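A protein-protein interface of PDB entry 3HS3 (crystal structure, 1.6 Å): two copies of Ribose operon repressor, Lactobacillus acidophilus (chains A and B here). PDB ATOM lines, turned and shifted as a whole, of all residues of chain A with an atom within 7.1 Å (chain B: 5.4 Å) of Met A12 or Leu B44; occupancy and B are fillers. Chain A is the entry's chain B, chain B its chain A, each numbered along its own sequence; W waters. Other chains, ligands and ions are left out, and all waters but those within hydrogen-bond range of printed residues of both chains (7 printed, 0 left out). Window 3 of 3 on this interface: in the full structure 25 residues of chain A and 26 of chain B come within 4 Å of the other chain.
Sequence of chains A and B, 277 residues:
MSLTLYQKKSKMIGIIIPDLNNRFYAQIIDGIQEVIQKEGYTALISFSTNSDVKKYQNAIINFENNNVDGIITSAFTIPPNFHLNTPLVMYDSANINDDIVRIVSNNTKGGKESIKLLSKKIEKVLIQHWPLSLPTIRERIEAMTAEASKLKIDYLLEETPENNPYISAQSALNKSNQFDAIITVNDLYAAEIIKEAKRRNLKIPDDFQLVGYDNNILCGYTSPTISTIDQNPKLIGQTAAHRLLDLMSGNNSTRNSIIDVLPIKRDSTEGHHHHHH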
ATOM      1  N   LYS A   9      -6.714  -5.988  20.164  1.00  0.00           N
ATOM      2  CA  LYS A   9      -6.603  -6.802  21.367  1.00  0.00           C
ATOM      3  C   LYS A   9      -6.834  -8.284  21.079  1.00  0.00           C
ATOM      4  O   LYS A   9      -7.627  -8.649  20.207  1.00  0.00           O
ATOM      5  CB  LYS A   9      -7.595  -6.305  22.418  1.00  0.00           C
ATOM      6  CG  LYS A   9      -7.395  -4.843  22.796  1.00  0.00           C
ATOM      7  CD  LYS A   9      -5.991  -4.592  23.334  1.00  0.00           C
ATOM      8  CE  LYS A   9      -5.778  -3.127  23.703  1.00  0.00           C
ATOM      9  NZ  LYS A   9      -5.933  -2.215  22.533  1.00  0.00           N
ATOM     10  N   SER A  10      -6.134  -9.132  21.827  1.00  0.00           N
ATOM     11  CA  SER A  10      -6.223 -10.579  21.665  1.00  0.00           C
ATOM     12  C   SER A  10      -7.144 -11.235  22.683  1.00  0.00           C
ATOM     13  O   SER A  10      -7.556 -12.384  22.506  1.00  0.00           O
ATOM     14  CB  SER A  10      -4.836 -11.198  21.815  1.00  0.00           C
ATOM     15  OG  SER A  10      -4.362 -11.004  23.141  1.00  0.00           O
ATOM     16  N   LYS A  11      -7.453 -10.510  23.749  1.00  0.00           N
ATOM     17  CA  LYS A  11      -8.285 -11.042  24.818  1.00  0.00           C
ATOM     18  C   LYS A  11      -7.589 -12.247  25.456  1.00  0.00           C
ATOM     19  O   LYS A  11      -8.238 -13.190  25.905  1.00  0.00           O
ATOM     20  CB  LYS A  11      -9.676 -11.437  24.296  1.00  0.00           C
ATOM     21  CG  LYS A  11     -10.540 -10.253  23.868  1.00  0.00           C
ATOM     22  CD  LYS A  11     -10.719  -9.232  24.994  1.00  0.00           C
ATOM     23  CE  LYS A  11     -11.645  -9.728  26.102  1.00  0.00           C
ATOM     24  NZ  LYS A  11     -13.073  -9.815  25.674  1.00  0.00           N
ATOM     25  N   MET A  12      -6.259 -12.209  25.465  1.00  0.00           N
ATOM     26  CA  MET A  12      -5.450 -13.252  26.088  1.00  0.00           C
ATOM     27  C   MET A  12      -4.605 -12.567  27.150  1.00  0.00           C
ATOM     28  O   MET A  12      -4.144 -11.441  26.957  1.00  0.00           O
ATOM     29  CB  MET A  12      -4.502 -13.934  25.086  1.00  0.00           C
ATOM     30  CG  MET A  12      -5.149 -14.944  24.145  1.00  0.00           C
ATOM     31  SD  MET A  12      -3.923 -15.763  23.059  1.00  0.00           S
ATOM     32  CE  MET A  12      -3.868 -14.621  21.720  1.00  0.00           C
ATOM     33  N   ILE A  13      -4.408 -13.248  28.272  1.00  0.00           N
ATOM     34  CA  ILE A  13      -3.592 -12.720  29.351  1.00  0.00           C
ATOM     35  C   ILE A  13      -2.487 -13.727  29.600  1.00  0.00           C
ATOM     36  O   ILE A  13      -2.757 -14.904  29.851  1.00  0.00           O
ATOM     37  CB  ILE A  13      -4.399 -12.556  30.656  1.00  0.00           C
ATOM     38  CG1 ILE A  13      -5.494 -11.505  30.468  1.00  0.00           C
ATOM     39  CG2 ILE A  13      -3.473 -12.162  31.808  1.00  0.00           C
ATOM     40  CD1 ILE A  13      -4.969 -10.128  30.167  1.00  0.00           C
ATOM     41  N   GLY A  14      -1.243 -13.276  29.506  1.00  0.00           N
ATOM     42  CA  GLY A  14      -0.136 -14.178  29.753  1.00  0.00           C
ATOM     43  C   GLY A  14       0.077 -14.340  31.246  1.00  0.00           C
ATOM     44  O   GLY A  14       0.037 -13.360  31.995  1.00  0.00           O
ATOM     45  N   ILE A  36     -10.688 -12.859  35.125  1.00  0.00           N
ATOM     46  CA  ILE A  36     -10.511 -12.572  33.706  1.00  0.00           C
ATOM     47  C   ILE A  36     -11.428 -13.326  32.754  1.00  0.00           C
ATOM     48  O   ILE A  36     -11.777 -12.795  31.698  1.00  0.00           O
ATOM     49  CB  ILE A  36      -9.036 -12.763  33.255  1.00  0.00           C
ATOM     50  CG1 ILE A  36      -8.664 -14.245  33.207  1.00  0.00           C
ATOM     51  CG2 ILE A  36      -8.108 -12.021  34.213  1.00  0.00           C
ATOM     52  CD1 ILE A  36      -7.332 -14.487  32.532  1.00  0.00           C
ATOM     53  N   GLY A  40     -14.214 -12.290  29.432  1.00  0.00           N
ATOM     54  CA  GLY A  40     -13.929 -12.807  28.104  1.00  0.00           C
ATOM     55  C   GLY A  40     -12.481 -13.075  27.745  1.00  0.00           C
ATOM     56  O   GLY A  40     -12.162 -13.271  26.570  1.00  0.00           O
ATOM     57  N   TYR A  41     -11.604 -13.086  28.743  1.00  0.00           N
ATOM     58  CA  TYR A  41     -10.187 -13.346  28.506  1.00  0.00           C
ATOM     59  C   TYR A  41      -9.852 -14.819  28.691  1.00  0.00           C
ATOM     60  O   TYR A  41     -10.528 -15.532  29.436  1.00  0.00           O
ATOM     61  CB  TYR A  41      -9.327 -12.530  29.475  1.00  0.00           C
ATOM     62  CG  TYR A  41      -9.335 -11.048  29.210  1.00  0.00           C
ATOM     63  CD1 TYR A  41      -8.444 -10.478  28.303  1.00  0.00           C
ATOM     64  CD2 TYR A  41     -10.249 -10.217  29.848  1.00  0.00           C
ATOM     65  CE1 TYR A  41      -8.467  -9.107  28.036  1.00  0.00           C
ATOM     66  CE2 TYR A  41     -10.281  -8.853  29.591  1.00  0.00           C
ATOM     67  CZ  TYR A  41      -9.391  -8.303  28.685  1.00  0.00           C
ATOM     68  OH  TYR A  41      -9.450  -6.953  28.423  1.00  0.00           O
ATOM     69  N   THR A  42      -8.813 -15.274  28.000  1.00  0.00           N
ATOM     70  CA  THR A  42      -8.350 -16.649  28.124  1.00  0.00           C
ATOM     71  C   THR A  42      -6.898 -16.575  28.573  1.00  0.00           C
ATOM     72  O   THR A  42      -6.123 -15.762  28.068  1.00  0.00           O
ATOM     73  CB  THR A  42      -8.418 -17.414  26.788  1.00  0.00           C
ATOM     74  OG1 THR A  42      -9.772 -17.441  26.322  1.00  0.00           O
ATOM     75  CG2 THR A  42      -7.930 -18.851  26.978  1.00  0.00           C
ATOM     76  N   ALA A  43      -6.539 -17.421  29.527  1.00  0.00           N
ATOM     77  CA  ALA A  43      -5.183 -17.449  30.052  1.00  0.00           C
ATOM     78  C   ALA A  43      -4.204 -18.203  29.157  1.00  0.00           C
ATOM     79  O   ALA A  43      -4.458 -19.340  28.749  1.00  0.00           O
ATOM     80  CB  ALA A  43      -5.191 -18.070  31.443  1.00  0.00           C
ATOM     81  N   LEU A  44      -3.093 -17.546  28.839  1.00  0.00           N
ATOM     82  CA  LEU A  44      -2.022 -18.147  28.044  1.00  0.00           C
ATOM     83  C   LEU A  44      -0.957 -18.345  29.116  1.00  0.00           C
ATOM     84  O   LEU A  44      -0.318 -17.387  29.558  1.00  0.00           O
ATOM     85  CB  LEU A  44      -1.538 -17.176  26.967  1.00  0.00           C
ATOM     86  CG  LEU A  44      -0.474 -17.708  26.004  1.00  0.00           C
ATOM     87  CD1 LEU A  44      -1.019 -18.871  25.188  1.00  0.00           C
ATOM     88  CD2 LEU A  44      -0.032 -16.581  25.078  1.00  0.00           C
ATOM     89  N   ILE A  45      -0.769 -19.591  29.536  1.00  0.00           N
ATOM     90  CA  ILE A  45       0.148 -19.882  30.630  1.00  0.00           C
ATOM     91  C   ILE A  45       1.465 -20.561  30.298  1.00  0.00           C
ATOM     92  O   ILE A  45       1.499 -21.591  29.627  1.00  0.00           O
ATOM     93  CB  ILE A  45      -0.581 -20.734  31.690  1.00  0.00           C
ATOM     94  CG1 ILE A  45      -1.920 -20.069  32.035  1.00  0.00           C
ATOM     95  CG2 ILE A  45       0.295 -20.901  32.932  1.00  0.00           C
ATOM     96  CD1 ILE A  45      -2.743 -20.825  33.064  1.00  0.00           C
ATOM     97  N   ASN A  66       2.992 -12.866  20.985  1.00  0.00           N
ATOM     98  CA  ASN A  66       1.662 -13.456  20.845  1.00  0.00           C
ATOM     99  C   ASN A  66       0.560 -12.422  21.090  1.00  0.00           C
ATOM    100  O   ASN A  66      -0.626 -12.755  21.163  1.00  0.00           O
ATOM    101  CB  ASN A  66       1.510 -14.641  21.804  1.00  0.00           C
ATOM    102  CG  ASN A  66       2.026 -15.937  21.206  1.00  0.00           C
ATOM    103  OD1 ASN A  66       2.528 -16.807  21.912  1.00  0.00           O
ATOM    104  ND2 ASN A  66       1.886 -16.076  19.892  1.00  0.00           N
ATOM    105  N   ASN A  67       0.972 -11.168  21.225  1.00  0.00           N
ATOM    106  CA  ASN A  67       0.060 -10.051  21.423  1.00  0.00           C
ATOM    107  C   ASN A  67      -0.906 -10.156  22.602  1.00  0.00           C
ATOM    108  O   ASN A  67      -2.077  -9.784  22.485  1.00  0.00           O
ATOM    109  CB  ASN A  67      -0.736  -9.804  20.135  1.00  0.00           C
ATOM    110  CG  ASN A  67      -1.520  -8.506  20.173  1.00  0.00           C
ATOM    111  OD1 ASN A  67      -0.993  -7.466  20.567  1.00  0.00           O
ATOM    112  ND2 ASN A  67      -2.782  -8.558  19.754  1.00  0.00           N
ATOM    113  N   VAL A  68      -0.441 -10.659  23.740  1.00  0.00           N
ATOM    114  CA  VAL A  68      -1.326 -10.730  24.900  1.00  0.00           C
ATOM    115  C   VAL A  68      -1.657  -9.295  25.319  1.00  0.00           C
ATOM    116  O   VAL A  68      -0.890  -8.365  25.041  1.00  0.00           O
ATOM    117  CB  VAL A  68      -0.668 -11.468  26.091  1.00  0.00           C
ATOM    118  CG1 VAL A  68      -0.398 -12.921  25.718  1.00  0.00           C
ATOM    119  CG2 VAL A  68       0.614 -10.765  26.497  1.00  0.00           C
ATOM    120  N   ASP A  69      -2.796  -9.110  25.977  1.00  0.00           N
ATOM    121  CA  ASP A  69      -3.212  -7.773  26.403  1.00  0.00           C
ATOM    122  C   ASP A  69      -2.620  -7.353  27.749  1.00  0.00           C
ATOM    123  O   ASP A  69      -2.593  -6.164  28.088  1.00  0.00           O
ATOM    124  CB  ASP A  69      -4.741  -7.700  26.472  1.00  0.00           C
ATOM    125  CG  ASP A  69      -5.399  -7.952  25.130  1.00  0.00           C
ATOM    126  OD1 ASP A  69      -4.696  -7.907  24.098  1.00  0.00           O
ATOM    127  OD2 ASP A  69      -6.627  -8.188  25.112  1.00  0.00           O
ATOM    128  N   GLY A  70      -2.146  -8.337  28.510  1.00  0.00           N
ATOM    129  CA  GLY A  70      -1.563  -8.066  29.808  1.00  0.00           C
ATOM    130  C   GLY A  70      -0.818  -9.294  30.280  1.00  0.00           C
ATOM    131  O   GLY A  70      -1.035 -10.392  29.760  1.00  0.00           O
ATOM    132  N   ILE A  71       0.060  -9.115  31.262  1.00  0.00           N
ATOM    133  CA  ILE A  71       0.852 -10.223  31.782  1.00  0.00           C
ATOM    134  C   ILE A  71       0.870 -10.222  33.300  1.00  0.00           C
ATOM    135  O   ILE A  71       1.008  -9.173  33.930  1.00  0.00           O
ATOM    136  CB  ILE A  71       2.317 -10.133  31.292  1.00  0.00           C
ATOM    137  CG1 ILE A  71       2.366 -10.283  29.770  1.00  0.00           C
ATOM    138  CG2 ILE A  71       3.170 -11.203  31.971  1.00  0.00           C
ATOM    139  CD1 ILE A  71       3.714  -9.915  29.150  1.00  0.00           C
ATOM    140  N   LEU A 244      -4.404  -5.702  37.070  1.00  0.00           N
ATOM    141  CA  LEU A 244      -3.972  -5.781  35.677  1.00  0.00           C
ATOM    142  C   LEU A 244      -5.022  -5.124  34.780  1.00  0.00           C
ATOM    143  O   LEU A 244      -4.679  -4.391  33.854  1.00  0.00           O
ATOM    144  CB  LEU A 244      -3.763  -7.231  35.230  1.00  0.00           C
ATOM    145  CG  LEU A 244      -3.246  -7.334  33.784  1.00  0.00           C
ATOM    146  CD1 LEU A 244      -1.811  -6.815  33.720  1.00  0.00           C
ATOM    147  CD2 LEU A 244      -3.321  -8.772  33.295  1.00  0.00           C
ATOM    148  N   MET A 248      -4.639  -1.967  32.212  1.00  0.00           N
ATOM    149  CA  MET A 248      -5.094  -2.110  30.837  1.00  0.00           C
ATOM    150  C   MET A 248      -6.167  -1.069  30.528  1.00  0.00           C
ATOM    151  O   MET A 248      -6.619  -0.946  29.384  1.00  0.00           O
ATOM    152  CB  MET A 248      -5.653  -3.520  30.624  1.00  0.00           C
ATOM    153  CG  MET A 248      -4.603  -4.633  30.685  1.00  0.00           C
ATOM    154  SD  MET A 248      -5.283  -6.314  30.847  1.00  0.00           S
ATOM    155  CE  MET A 248      -6.555  -6.288  29.552  1.00  0.00           C
ATOM    156  N   MET B  12       0.361 -22.869  19.819  1.00  0.00           N
ATOM    157  CA  MET B  12      -0.448 -22.815  21.036  1.00  0.00           C
ATOM    158  C   MET B  12      -1.279 -24.092  21.082  1.00  0.00           C
ATOM    159  O   MET B  12      -1.742 -24.582  20.047  1.00  0.00           O
ATOM    160  CB  MET B  12      -1.410 -21.617  21.034  1.00  0.00           C
ATOM    161  CG  MET B  12      -0.773 -20.251  21.254  1.00  0.00           C
ATOM    162  SD  MET B  12      -2.008 -18.916  21.424  1.00  0.00           S
ATOM    163  CE  MET B  12      -2.529 -18.740  19.774  1.00  0.00           C
ATOM    164  N   ILE B  13      -1.454 -24.636  22.281  1.00  0.00           N
ATOM    165  CA  ILE B  13      -2.251 -25.842  22.473  1.00  0.00           C
ATOM    166  C   ILE B  13      -3.351 -25.490  23.459  1.00  0.00           C
ATOM    167  O   ILE B  13      -3.074 -25.011  24.562  1.00  0.00           O
ATOM    168  CB  ILE B  13      -1.427 -27.001  23.084  1.00  0.00           C
ATOM    169  CG1 ILE B  13      -0.288 -27.386  22.142  1.00  0.00           C
ATOM    170  CG2 ILE B  13      -2.334 -28.209  23.346  1.00  0.00           C
ATOM    171  CD1 ILE B  13      -0.753 -27.906  20.817  1.00  0.00           C
ATOM    172  N   GLY B  14      -4.598 -25.708  23.061  1.00  0.00           N
ATOM    173  CA  GLY B  14      -5.697 -25.408  23.958  1.00  0.00           C
ATOM    174  C   GLY B  14      -5.871 -26.539  24.955  1.00  0.00           C
ATOM    175  O   GLY B  14      -5.820 -27.710  24.579  1.00  0.00           O
ATOM    176  N   ILE B  15      -6.063 -26.195  26.224  1.00  0.00           N
ATOM    177  CA  ILE B  15      -6.258 -27.207  27.255  1.00  0.00           C
ATOM    178  C   ILE B  15      -7.443 -26.832  28.120  1.00  0.00           C
ATOM    179  O   ILE B  15      -7.574 -25.682  28.531  1.00  0.00           O
ATOM    180  CB  ILE B  15      -5.035 -27.325  28.189  1.00  0.00           C
ATOM    181  CG1 ILE B  15      -3.770 -27.575  27.374  1.00  0.00           C
ATOM    182  CG2 ILE B  15      -5.257 -28.462  29.187  1.00  0.00           C
ATOM    183  CD1 ILE B  15      -2.507 -27.611  28.218  1.00  0.00           C
ATOM    184  N   THR B  42       2.946 -23.225  23.720  1.00  0.00           N
ATOM    185  CA  THR B  42       2.498 -22.541  24.926  1.00  0.00           C
ATOM    186  C   THR B  42       1.056 -22.972  25.150  1.00  0.00           C
ATOM    187  O   THR B  42       0.274 -23.078  24.202  1.00  0.00           O
ATOM    188  CB  THR B  42       2.545 -21.009  24.788  1.00  0.00           C
ATOM    189  OG1 THR B  42       3.901 -20.593  24.590  1.00  0.00           O
ATOM    190  CG2 THR B  42       2.002 -20.342  26.051  1.00  0.00           C
ATOM    191  N   ALA B  43       0.709 -23.227  26.403  1.00  0.00           N
ATOM    192  CA  ALA B  43      -0.631 -23.666  26.744  1.00  0.00           C
ATOM    193  C   ALA B  43      -1.637 -22.528  26.864  1.00  0.00           C
ATOM    194  O   ALA B  43      -1.395 -21.538  27.557  1.00  0.00           O
ATOM    195  CB  ALA B  43      -0.589 -24.450  28.051  1.00  0.00           C
ATOM    196  N   LEU B  44      -2.763 -22.679  26.172  1.00  0.00           N
ATOM    197  CA  LEU B  44      -3.857 -21.713  26.226  1.00  0.00           C
ATOM    198  C   LEU B  44      -4.879 -22.507  27.032  1.00  0.00           C
ATOM    199  O   LEU B  44      -5.501 -23.440  26.515  1.00  0.00           O
ATOM    200  CB  LEU B  44      -4.390 -21.424  24.822  1.00  0.00           C
ATOM    201  CG  LEU B  44      -5.421 -20.298  24.687  1.00  0.00           C
ATOM    202  CD1 LEU B  44      -4.847 -18.963  25.172  1.00  0.00           C
ATOM    203  CD2 LEU B  44      -5.823 -20.193  23.230  1.00  0.00           C
ATOM    204  N   ILE B  45      -5.047 -22.145  28.298  1.00  0.00           N
ATOM    205  CA  ILE B  45      -5.925 -22.903  29.178  1.00  0.00           C
ATOM    206  C   ILE B  45      -7.242 -22.260  29.576  1.00  0.00           C
ATOM    207  O   ILE B  45      -7.288 -21.103  29.995  1.00  0.00           O
ATOM    208  CB  ILE B  45      -5.159 -23.279  30.465  1.00  0.00           C
ATOM    209  CG1 ILE B  45      -3.844 -23.971  30.090  1.00  0.00           C
ATOM    210  CG2 ILE B  45      -6.001 -24.190  31.344  1.00  0.00           C
ATOM    211  CD1 ILE B  45      -2.950 -24.288  31.273  1.00  0.00           C
ATOM    212  N   SER B  46      -8.314 -23.035  29.449  1.00  0.00           N
ATOM    213  CA  SER B  46      -9.642 -22.576  29.830  1.00  0.00           C
ATOM    214  C   SER B  46     -10.078 -23.416  31.022  1.00  0.00           C
ATOM    215  O   SER B  46      -9.982 -24.642  31.004  1.00  0.00           O
ATOM    216  CB  SER B  46     -10.628 -22.739  28.670  1.00  0.00           C
ATOM    217  OG  SER B  46     -10.328 -21.829  27.619  1.00  0.00           O
ATOM    218  N   PHE B  63     -11.158 -21.842  21.187  1.00  0.00           N
ATOM    219  CA  PHE B  63      -9.775 -22.235  20.941  1.00  0.00           C
ATOM    220  C   PHE B  63      -9.517 -22.173  19.443  1.00  0.00           C
ATOM    221  O   PHE B  63      -8.472 -21.702  19.002  1.00  0.00           O
ATOM    222  CB  PHE B  63      -9.498 -23.669  21.405  1.00  0.00           C
ATOM    223  CG  PHE B  63      -9.319 -23.818  22.891  1.00  0.00           C
ATOM    224  CD1 PHE B  63      -8.795 -22.781  23.660  1.00  0.00           C
ATOM    225  CD2 PHE B  63      -9.598 -25.038  23.506  1.00  0.00           C
ATOM    226  CE1 PHE B  63      -8.564 -22.952  25.029  1.00  0.00           C
ATOM    227  CE2 PHE B  63      -9.372 -25.225  24.877  1.00  0.00           C
ATOM    228  CZ  PHE B  63      -8.846 -24.182  25.635  1.00  0.00           C
ATOM    229  N   ASN B  66      -8.910 -18.938  18.035  1.00  0.00           N
ATOM    230  CA  ASN B  66      -7.567 -18.468  18.352  1.00  0.00           C
ATOM    231  C   ASN B  66      -6.491 -19.256  17.612  1.00  0.00           C
ATOM    232  O   ASN B  66      -5.296 -19.128  17.885  1.00  0.00           O
ATOM    233  CB  ASN B  66      -7.328 -18.505  19.864  1.00  0.00           C
ATOM    234  CG  ASN B  66      -7.917 -17.297  20.567  1.00  0.00           C
ATOM    235  OD1 ASN B  66      -7.700 -16.161  20.145  1.00  0.00           O
ATOM    236  ND2 ASN B  66      -8.656 -17.531  21.644  1.00  0.00           N
ATOM    237  N   VAL B  68      -5.532 -22.425  17.637  1.00  0.00           N
ATOM    238  CA  VAL B  68      -4.637 -23.331  18.353  1.00  0.00           C
ATOM    239  C   VAL B  68      -4.313 -24.483  17.404  1.00  0.00           C
ATOM    240  O   VAL B  68      -5.108 -24.796  16.514  1.00  0.00           O
ATOM    241  CB  VAL B  68      -5.287 -23.896  19.641  1.00  0.00           C
ATOM    242  CG1 VAL B  68      -5.614 -22.759  20.596  1.00  0.00           C
ATOM    243  CG2 VAL B  68      -6.536 -24.692  19.300  1.00  0.00           C
HETATM  244  O   HOH W   1      -9.172 -14.747  22.972  1.00  0.00           O
HETATM  245  O   HOH W   2     -11.072 -19.362  28.631  1.00  0.00           O
HETATM  246  O   HOH W   3       4.161 -17.530  24.455  1.00  0.00           O
HETATM  247  O   HOH W   4      -7.202 -13.539  20.034  1.00  0.00           O
HETATM  248  O   HOH W   5       2.919 -23.188  28.130  1.00  0.00           O
HETATM  249  O   HOH W   6     -10.005 -19.183  23.903  1.00  0.00           O
HETATM  250  O   HOH W   7      -8.727 -18.986  30.615  1.00  0.00           O
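The backbone carbonyl oxygen (O) of Ala B43 is in hydrogen-bond range of the backbone NH (N) of Ile A45 (2.8 Å).
The backbone NH of Ile B45 is in hydrogen-bond range of the backbone carbonyl oxygen of Ala A43, 2.9 Å away.
The backbone carbonyl oxygen (O) of Ile B13 lies within hydrogen-bond range of the backbone NH (N) of Leu B44, 2.9 Å away.
N of Ile B15 is in hydrogen-bond range of O of Leu B44, at 2.8 Å.
O of Ile B15 is in hydrogen-bond range of N of Ser B46 (2.9 Å).
The backbone NH of Met A12 lies close to the side-chain hydroxyl of Ser A10, 3.2 Å away.
O of Met A12 sits at hydrogen-bond distance from N of Asp A69 (2.9 Å).
The backbone carbonyl oxygen (O) of Thr A42 sits at hydrogen-bond distance from the backbone NH (N) of Ile A13 (3.1 Å).
Among the printed residues, pairs that only touch across the chains: Leu A44 with Thr B42, Leu A44 with Ala B43, Ala A43 with Leu B44, Thr A42 with Leu B44, Thr A42 with Ile B45, Ile A45 with Thr B42, Leu A44 with Leu B44, Thr A42 with Ser B46, Leu A44 with Met B12, Ile A45 with Ile B45, Met A12 with Leu B44 and Ala A43 with Ala B43.
Printed residues of chain B within 4 Å of Met A12: Leu B44 (3.9 Å).
Of chain A, only Met A12, Thr A42, Ala A43 and Leu A44 come within 4 Å of Leu B44.
Of the printed residues of chain A, Thr B42 touches Leu A44 and Ile A45.
Printed residues of chain A within 4 Å of Met B12: Leu A44.
Asn B66 touches none of the printed residues of chain A.
Ser A10 touches none of the printed residues of chain B.
The nearest residue of chain A that does not touch Leu B44 is Ile A45 (5.0 Å).
The nearest printed residue of chain B that does not touch Ile A45 is Leu B44 (5.0 Å).
Hydrophobic or aromatic side chains of chain B within 4 Å of the printed part of chain A: Met B12, Ala B43, Leu B44 and Ile B45.
Hydrophobic or aromatic side chains of chain A that line the printed part of chain B: Met A12, Ala A43, Leu A44 and Ile A45.
Among the printed residues, no Asp or Glu carboxylate lies within 4 Å of a Lys or Arg side-chain nitrogen of the other chain.
Met A12 touches Leu B44, and with the chains exchanged Leu A44 touches Met B12.
Thr A42 touches Leu B44, and with the chains exchanged Leu A44 touches Thr B42.
Ala A43 touches Leu B44, and with the chains exchanged Leu A44 touches Ala B43.
Leu B44 touches its own counterpart, Leu A44.
Of the 14 pairs that touch across the chains among the printed residues, 13 have their exchanged pair printed and touching as well.
Water W5 bridges the backbone carbonyl oxygen of Ile A45 (2.6 Å) and the backbone NH of Ala B43 (2.8 Å).
Water W4 bridges the side-chain amide oxygen of Asn B66 (2.7 Å) and the backbone carbonyl oxygen of Ser A10 (2.8 Å).
Water W2 lies within hydrogen-bond range of OG of Ser B46 (2.8 Å) and OG1 of Thr A42 (3.3 Å).
Water W1 lies within hydrogen-bond range of the backbone carbonyl oxygen (O) of Ser A10 (2.9 Å), the side-chain amide nitrogen (ND2) of Asn B66 (3.1 Å) and the backbone carbonyl oxygen (O) of Lys A11 (3.4 Å).
Water W6 bridges the side-chain hydroxyl of Thr A42 and the side-chain amide nitrogen of Asn B66.
Water W3 lies within hydrogen-bond range of the side-chain hydroxyl (OG1) of Thr B42 (3.1 Å) and the side-chain amide oxygen (OD1) of Asn A66 (3.1 Å).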
